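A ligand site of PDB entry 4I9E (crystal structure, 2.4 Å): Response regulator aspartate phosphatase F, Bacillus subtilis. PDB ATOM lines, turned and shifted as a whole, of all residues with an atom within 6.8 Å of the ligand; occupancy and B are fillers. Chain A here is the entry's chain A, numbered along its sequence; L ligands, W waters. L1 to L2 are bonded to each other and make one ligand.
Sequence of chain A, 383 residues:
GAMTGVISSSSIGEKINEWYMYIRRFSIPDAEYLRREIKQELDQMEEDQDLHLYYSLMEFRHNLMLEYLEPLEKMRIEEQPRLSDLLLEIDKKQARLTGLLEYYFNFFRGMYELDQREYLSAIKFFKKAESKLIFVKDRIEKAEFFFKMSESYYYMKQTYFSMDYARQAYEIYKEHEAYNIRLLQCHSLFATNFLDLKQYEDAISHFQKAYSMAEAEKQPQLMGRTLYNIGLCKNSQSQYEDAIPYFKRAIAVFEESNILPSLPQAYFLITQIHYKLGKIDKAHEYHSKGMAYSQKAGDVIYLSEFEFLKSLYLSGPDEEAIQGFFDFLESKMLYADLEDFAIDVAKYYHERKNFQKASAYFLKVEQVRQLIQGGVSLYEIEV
Water W1 bridges the backbone carbonyl oxygen of Pro 261 (3.1 Å) and an oxygen (O6) of LG2 L2 (3.4 Å). Water W2 lies within hydrogen-bond range of the side-chain carboxylate (OD1) of Asp 337 (2.7 Å), the backbone NH (N) of Gly 1 (2.8 Å) and an oxygen (O2) of LIG L1 (3.4 Å).
The backbone carbonyl oxygen (O) of Gly 1 is in hydrogen-bond range of the side-chain amide nitrogen (NE2) of Gln 265, 2.8 Å away. NE2 of Gln 265 lies within hydrogen-bond range of OH of Tyr 228 (3.2 Å). The backbone NH (N) of Tyr 302 lies within hydrogen-bond range of the side-chain carboxylate (OD1) of Asp 299.
Merely in contact with the ligand: Ala 2 (3.2 Å), Met 3 (3.4 Å), Ile 301 (3.6 Å), Tyr 302 (3.3 Å) and Glu 305 (3.98 Å). Nine residues have an atom within 4 Å of the ligand: Gly 1, Ala 2, Met 3, Thr 4, Gln 265, Ile 301, Tyr 302, Glu 305 and Asp 337.
O3 of LIG L1 sits at hydrogen-bond distance from OD2 of Asp 337 (2.6 Å). N of Gly 1 is in hydrogen-bond range of O1 of LIG L1 (2.8 Å). The backbone carbonyl oxygen (O) of Gly 1 lies within hydrogen-bond range of an oxygen (O1) of LIG L1, 3.0 Å away. The backbone NH of Thr 4 lies within hydrogen-bond range of an oxygen (O1) of LG2 L2. The side-chain amide nitrogen (NE2) of Gln 265 sits at hydrogen-bond distance from an oxygen (O1) of LIG L1 (3.3 Å).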
ATOM      1  N   GLY A   1      19.760  -2.723  26.148  1.00  0.00           N
ATOM      2  CA  GLY A   1      21.243  -2.811  25.833  1.00  0.00           C
ATOM      3  C   GLY A   1      21.893  -1.454  26.082  1.00  0.00           C
ATOM      4  O   GLY A   1      21.285  -0.611  26.684  1.00  0.00           O
ATOM      5  N   ALA A   2      23.105  -1.224  25.594  1.00  0.00           N
ATOM      6  CA  ALA A   2      23.790   0.046  25.827  1.00  0.00           C
ATOM      7  C   ALA A   2      23.103   1.266  25.219  1.00  0.00           C
ATOM      8  O   ALA A   2      22.559   1.205  24.103  1.00  0.00           O
ATOM      9  CB  ALA A   2      25.302  -0.014  25.393  1.00  0.00           C
ATOM     10  N   MET A   3      23.145   2.368  25.952  1.00  0.00           N
ATOM     11  CA  MET A   3      22.677   3.631  25.419  1.00  0.00           C
ATOM     12  C   MET A   3      23.651   4.162  24.420  1.00  0.00           C
ATOM     13  O   MET A   3      24.835   4.380  24.721  1.00  0.00           O
ATOM     14  CB  MET A   3      22.566   4.656  26.517  1.00  0.00           C
ATOM     15  CG  MET A   3      21.275   4.587  27.133  1.00  0.00           C
ATOM     16  SD  MET A   3      21.097   5.963  28.195  1.00  0.00           S
ATOM     17  CE  MET A   3      19.689   5.404  29.116  1.00  0.00           C
ATOM     18  N   THR A   4      23.143   4.402  23.226  1.00  0.00           N
ATOM     19  CA  THR A   4      24.024   4.782  22.151  1.00  0.00           C
ATOM     20  C   THR A   4      24.215   6.310  21.929  1.00  0.00           C
ATOM     21  O   THR A   4      25.360   6.763  22.019  1.00  0.00           O
ATOM     22  CB  THR A   4      23.838   3.997  20.865  1.00  0.00           C
ATOM     23  OG1 THR A   4      24.513   4.720  19.832  1.00  0.00           O
ATOM     24  CG2 THR A   4      22.368   3.832  20.497  1.00  0.00           C
ATOM     25  N   GLY A   5      23.179   7.100  21.546  1.00  0.00           N
ATOM     26  CA  GLY A   5      22.111   6.740  20.585  1.00  0.00           C
ATOM     27  C   GLY A   5      21.628   7.964  19.790  1.00  0.00           C
ATOM     28  O   GLY A   5      22.326   9.005  19.749  1.00  0.00           O
ATOM     29  N   VAL A   6      20.470   7.791  19.112  1.00  0.00           N
ATOM     30  CA  VAL A   6      19.463   8.862  18.741  1.00  0.00           C
ATOM     31  C   VAL A   6      18.941   9.135  17.274  1.00  0.00           C
ATOM     32  O   VAL A   6      17.772   8.811  16.967  1.00  0.00           O
ATOM     33  CB  VAL A   6      19.579  10.213  19.572  1.00  0.00           C
ATOM     34  CG1 VAL A   6      18.591  11.263  19.058  1.00  0.00           C
ATOM     35  CG2 VAL A   6      19.258   9.947  21.025  1.00  0.00           C
ATOM     36  N   TYR A 155      25.730  -1.162  14.943  1.00  0.00           N
ATOM     37  CA  TYR A 155      24.364  -1.627  14.760  1.00  0.00           C
ATOM     38  C   TYR A 155      24.296  -2.999  14.066  1.00  0.00           C
ATOM     39  O   TYR A 155      23.413  -3.817  14.369  1.00  0.00           O
ATOM     40  CB  TYR A 155      23.528  -0.592  14.004  1.00  0.00           C
ATOM     41  CG  TYR A 155      23.503   0.764  14.643  1.00  0.00           C
ATOM     42  CD1 TYR A 155      23.433   0.907  16.046  1.00  0.00           C
ATOM     43  CD2 TYR A 155      23.528   1.916  13.859  1.00  0.00           C
ATOM     44  CE1 TYR A 155      23.421   2.150  16.621  1.00  0.00           C
ATOM     45  CE2 TYR A 155      23.511   3.190  14.437  1.00  0.00           C
ATOM     46  CZ  TYR A 155      23.450   3.288  15.820  1.00  0.00           C
ATOM     47  OH  TYR A 155      23.406   4.545  16.400  1.00  0.00           O
ATOM     48  N   ARG A 225      24.655   8.984  29.718  1.00  0.00           N
ATOM     49  CA  ARG A 225      24.726   7.791  28.915  1.00  0.00           C
ATOM     50  C   ARG A 225      25.862   6.849  29.332  1.00  0.00           C
ATOM     51  O   ARG A 225      25.670   5.659  29.403  1.00  0.00           O
ATOM     52  CB  ARG A 225      24.847   8.173  27.464  1.00  0.00           C
ATOM     53  CG  ARG A 225      23.503   8.515  26.876  1.00  0.00           C
ATOM     54  CD  ARG A 225      23.607   8.533  25.407  1.00  0.00           C
ATOM     55  NE  ARG A 225      22.498   9.308  24.880  1.00  0.00           N
ATOM     56  CZ  ARG A 225      21.604   8.880  23.995  1.00  0.00           C
ATOM     57  NH1 ARG A 225      21.689   7.649  23.473  1.00  0.00           N
ATOM     58  NH2 ARG A 225      20.621   9.705  23.630  1.00  0.00           N
ATOM     59  N   TYR A 228      25.208   5.378  32.813  1.00  0.00           N
ATOM     60  CA  TYR A 228      24.274   4.276  32.593  1.00  0.00           C
ATOM     61  C   TYR A 228      24.993   3.056  32.028  1.00  0.00           C
ATOM     62  O   TYR A 228      24.780   1.922  32.479  1.00  0.00           O
ATOM     63  CB  TYR A 228      23.153   4.696  31.643  1.00  0.00           C
ATOM     64  CG  TYR A 228      22.266   3.506  31.295  1.00  0.00           C
ATOM     65  CD1 TYR A 228      21.115   3.216  32.035  1.00  0.00           C
ATOM     66  CD2 TYR A 228      22.618   2.628  30.222  1.00  0.00           C
ATOM     67  CE1 TYR A 228      20.325   2.083  31.751  1.00  0.00           C
ATOM     68  CE2 TYR A 228      21.817   1.507  29.933  1.00  0.00           C
ATOM     69  CZ  TYR A 228      20.687   1.244  30.719  1.00  0.00           C
ATOM     70  OH  TYR A 228      19.901   0.165  30.417  1.00  0.00           O
ATOM     71  N   LEU A 232      25.405  -0.806  33.390  1.00  0.00           N
ATOM     72  CA  LEU A 232      25.001  -1.926  32.566  1.00  0.00           C
ATOM     73  C   LEU A 232      26.078  -2.977  32.563  1.00  0.00           C
ATOM     74  O   LEU A 232      25.796  -4.138  32.677  1.00  0.00           O
ATOM     75  CB  LEU A 232      24.672  -1.479  31.146  1.00  0.00           C
ATOM     76  CG  LEU A 232      23.688  -2.268  30.253  1.00  0.00           C
ATOM     77  CD1 LEU A 232      23.839  -1.844  28.844  1.00  0.00           C
ATOM     78  CD2 LEU A 232      23.901  -3.708  30.214  1.00  0.00           C
ATOM     79  N   PRO A 261      13.640  11.644  26.911  1.00  0.00           N
ATOM     80  CA  PRO A 261      13.856  10.483  26.052  1.00  0.00           C
ATOM     81  C   PRO A 261      14.675   9.352  26.718  1.00  0.00           C
ATOM     82  O   PRO A 261      14.357   8.171  26.545  1.00  0.00           O
ATOM     83  CB  PRO A 261      14.634  11.090  24.880  1.00  0.00           C
ATOM     84  CG  PRO A 261      14.031  12.524  24.788  1.00  0.00           C
ATOM     85  CD  PRO A 261      14.016  12.906  26.207  1.00  0.00           C
ATOM     86  N   GLN A 265      14.466   4.179  29.923  1.00  0.00           N
ATOM     87  CA  GLN A 265      15.600   3.234  30.005  1.00  0.00           C
ATOM     88  C   GLN A 265      16.452   3.447  31.263  1.00  0.00           C
ATOM     89  O   GLN A 265      16.824   2.469  31.915  1.00  0.00           O
ATOM     90  CB  GLN A 265      16.518   3.283  28.765  1.00  0.00           C
ATOM     91  CG  GLN A 265      17.559   2.097  28.630  1.00  0.00           C
ATOM     92  CD  GLN A 265      18.535   2.214  27.414  1.00  0.00           C
ATOM     93  OE1 GLN A 265      18.346   3.004  26.472  1.00  0.00           O
ATOM     94  NE2 GLN A 265      19.580   1.427  27.456  1.00  0.00           N
ATOM     95  N   ASP A 299       6.445   5.849  25.138  1.00  0.00           N
ATOM     96  CA  ASP A 299       7.395   4.762  24.868  1.00  0.00           C
ATOM     97  C   ASP A 299       6.646   3.416  24.940  1.00  0.00           C
ATOM     98  O   ASP A 299       6.504   2.787  25.998  1.00  0.00           O
ATOM     99  CB  ASP A 299       8.552   4.807  25.895  1.00  0.00           C
ATOM    100  CG  ASP A 299       9.886   4.341  25.316  1.00  0.00           C
ATOM    101  OD1 ASP A 299       9.942   3.287  24.644  1.00  0.00           O
ATOM    102  OD2 ASP A 299      10.913   5.043  25.496  1.00  0.00           O
ATOM    103  N   ILE A 301       7.640   0.556  23.780  1.00  0.00           N
ATOM    104  CA  ILE A 301       8.531  -0.536  24.125  1.00  0.00           C
ATOM    105  C   ILE A 301       8.799  -0.546  25.616  1.00  0.00           C
ATOM    106  O   ILE A 301       8.676  -1.594  26.233  1.00  0.00           O
ATOM    107  CB  ILE A 301       9.846  -0.525  23.284  1.00  0.00           C
ATOM    108  CG1 ILE A 301       9.525  -0.878  21.830  1.00  0.00           C
ATOM    109  CG2 ILE A 301      10.841  -1.577  23.830  1.00  0.00           C
ATOM    110  CD1 ILE A 301      10.611  -0.485  20.815  1.00  0.00           C
ATOM    111  N   TYR A 302       9.165   0.611  26.201  1.00  0.00           N
ATOM    112  CA  TYR A 302       9.299   0.635  27.657  1.00  0.00           C
ATOM    113  C   TYR A 302       8.019   0.444  28.515  1.00  0.00           C
ATOM    114  O   TYR A 302       8.090  -0.128  29.588  1.00  0.00           O
ATOM    115  CB  TYR A 302      10.189   1.784  28.119  1.00  0.00           C
ATOM    116  CG  TYR A 302      11.663   1.421  27.960  1.00  0.00           C
ATOM    117  CD1 TYR A 302      12.248   0.451  28.781  1.00  0.00           C
ATOM    118  CD2 TYR A 302      12.463   2.014  26.971  1.00  0.00           C
ATOM    119  CE1 TYR A 302      13.607   0.091  28.640  1.00  0.00           C
ATOM    120  CE2 TYR A 302      13.819   1.671  26.839  1.00  0.00           C
ATOM    121  CZ  TYR A 302      14.383   0.708  27.662  1.00  0.00           C
ATOM    122  OH  TYR A 302      15.699   0.351  27.543  1.00  0.00           O
ATOM    123  N   GLU A 305       7.755  -3.218  28.601  1.00  0.00           N
ATOM    124  CA  GLU A 305       8.850  -3.768  29.410  1.00  0.00           C
ATOM    125  C   GLU A 305       8.716  -3.541  30.917  1.00  0.00           C
ATOM    126  O   GLU A 305       9.029  -4.414  31.681  1.00  0.00           O
ATOM    127  CB  GLU A 305      10.224  -3.286  28.882  1.00  0.00           C
ATOM    128  CG  GLU A 305      10.532  -3.970  27.589  1.00  0.00           C
ATOM    129  CD  GLU A 305      11.868  -3.642  26.965  1.00  0.00           C
ATOM    130  OE1 GLU A 305      12.786  -3.039  27.602  1.00  0.00           O
ATOM    131  OE2 GLU A 305      12.012  -4.077  25.814  1.00  0.00           O
ATOM    132  N   LEU A 329       7.734  -8.392  21.555  1.00  0.00           N
ATOM    133  CA  LEU A 329       9.160  -8.175  21.259  1.00  0.00           C
ATOM    134  C   LEU A 329       9.588  -8.851  19.975  1.00  0.00           C
ATOM    135  O   LEU A 329      10.236  -8.229  19.125  1.00  0.00           O
ATOM    136  CB  LEU A 329      10.049  -8.679  22.390  1.00  0.00           C
ATOM    137  CG  LEU A 329      10.018  -7.995  23.752  1.00  0.00           C
ATOM    138  CD1 LEU A 329      11.066  -8.672  24.599  1.00  0.00           C
ATOM    139  CD2 LEU A 329      10.198  -6.483  23.732  1.00  0.00           C
ATOM    140  N   LEU A 334      12.830  -7.171  18.405  1.00  0.00           N
ATOM    141  CA  LEU A 334      13.681  -6.799  19.561  1.00  0.00           C
ATOM    142  C   LEU A 334      14.248  -8.070  20.205  1.00  0.00           C
ATOM    143  O   LEU A 334      13.916  -8.421  21.330  1.00  0.00           O
ATOM    144  CB  LEU A 334      12.911  -5.953  20.599  1.00  0.00           C
ATOM    145  CG  LEU A 334      12.258  -4.672  20.067  1.00  0.00           C
ATOM    146  CD1 LEU A 334      11.153  -4.129  21.035  1.00  0.00           C
ATOM    147  CD2 LEU A 334      13.357  -3.643  19.740  1.00  0.00           C
ATOM    148  N   ALA A 336      17.382  -9.158  20.943  1.00  0.00           N
ATOM    149  CA  ALA A 336      18.325  -9.105  22.053  1.00  0.00           C
ATOM    150  C   ALA A 336      17.564  -8.954  23.361  1.00  0.00           C
ATOM    151  O   ALA A 336      17.814  -9.736  24.288  1.00  0.00           O
ATOM    152  CB  ALA A 336      19.381  -7.981  21.890  1.00  0.00           C
ATOM    153  N   ASP A 337      16.668  -7.965  23.454  1.00  0.00           N
ATOM    154  CA  ASP A 337      15.832  -7.774  24.645  1.00  0.00           C
ATOM    155  C   ASP A 337      15.086  -9.056  24.969  1.00  0.00           C
ATOM    156  O   ASP A 337      15.127  -9.514  26.072  1.00  0.00           O
ATOM    157  CB  ASP A 337      14.768  -6.703  24.415  1.00  0.00           C
ATOM    158  CG  ASP A 337      15.313  -5.292  24.453  1.00  0.00           C
ATOM    159  OD1 ASP A 337      16.483  -5.074  24.168  1.00  0.00           O
ATOM    160  OD2 ASP A 337      14.544  -4.364  24.756  1.00  0.00           O
ATOM    161  N   PHE A 341      15.435 -11.238  28.405  1.00  0.00           N
ATOM    162  CA  PHE A 341      14.266 -11.422  29.248  1.00  0.00           C
ATOM    163  C   PHE A 341      13.854 -12.891  29.466  1.00  0.00           C
ATOM    164  O   PHE A 341      13.475 -13.276  30.595  1.00  0.00           O
ATOM    165  CB  PHE A 341      13.104 -10.540  28.781  1.00  0.00           C
ATOM    166  CG  PHE A 341      13.336  -9.063  28.979  1.00  0.00           C
ATOM    167  CD1 PHE A 341      13.968  -8.599  30.157  1.00  0.00           C
ATOM    168  CD2 PHE A 341      12.918  -8.157  28.026  1.00  0.00           C
ATOM    169  CE1 PHE A 341      14.238  -7.222  30.321  1.00  0.00           C
ATOM    170  CE2 PHE A 341      13.147  -6.751  28.158  1.00  0.00           C
ATOM    171  CZ  PHE A 341      13.824  -6.273  29.278  1.00  0.00           C
HETATM  172  C1  LIG L   1      17.141   1.125  24.091  1.00  0.00           C
HETATM  173  C2  LIG L   1      17.539  -0.167  24.828  1.00  0.00           C
HETATM  174  C3  LIG L   1      16.756  -1.362  24.294  1.00  0.00           C
HETATM  175  C4  LIG L   1      15.240  -1.012  24.123  1.00  0.00           C
HETATM  176  C5  LIG L   1      15.020   0.299  23.326  1.00  0.00           C
HETATM  177  C6  LIG L   1      13.568   0.676  23.271  1.00  0.00           C
HETATM  178  O1  LIG L   1      18.978  -0.399  24.807  1.00  0.00           O
HETATM  179  O2  LIG L   1      16.917  -2.479  25.180  1.00  0.00           O
HETATM  180  O3  LIG L   1      14.541  -2.076  23.489  1.00  0.00           O
HETATM  181  O4  LIG L   1      15.716   1.368  23.973  1.00  0.00           O
HETATM  182  O5  LIG L   1      13.344   1.592  22.210  1.00  0.00           O
HETATM  183  C1  LG2 L   2      19.706   2.456  23.277  1.00  0.00           C
HETATM  184  C2  LG2 L   2      18.448   2.319  22.457  1.00  0.00           C
HETATM  185  C3  LG2 L   2      18.717   2.201  20.964  1.00  0.00           C
HETATM  186  C4  LG2 L   2      17.440   2.786  20.362  1.00  0.00           C
HETATM  187  C5  LG2 L   2      17.063   3.911  21.351  1.00  0.00           C
HETATM  188  C6  LG2 L   2      15.569   4.312  21.371  1.00  0.00           C
HETATM  189  O1  LG2 L   2      20.301   3.685  22.933  1.00  0.00           O
HETATM  190  O2  LG2 L   2      17.781   1.098  22.802  1.00  0.00           O
HETATM  191  O3  LG2 L   2      18.963   0.836  20.630  1.00  0.00           O
HETATM  192  O4  LG2 L   2      17.683   3.276  19.044  1.00  0.00           O
HETATM  193  O5  LG2 L   2      17.580   3.459  22.645  1.00  0.00           O
HETATM  194  O6  LG2 L   2      15.128   4.523  22.734  1.00  0.00           O
HETATM  195  O   HOH W   1      14.170   7.701  23.537  1.00  0.00           O
HETATM  196  O   HOH W   2      19.171  -5.021  24.694  1.00  0.00           O
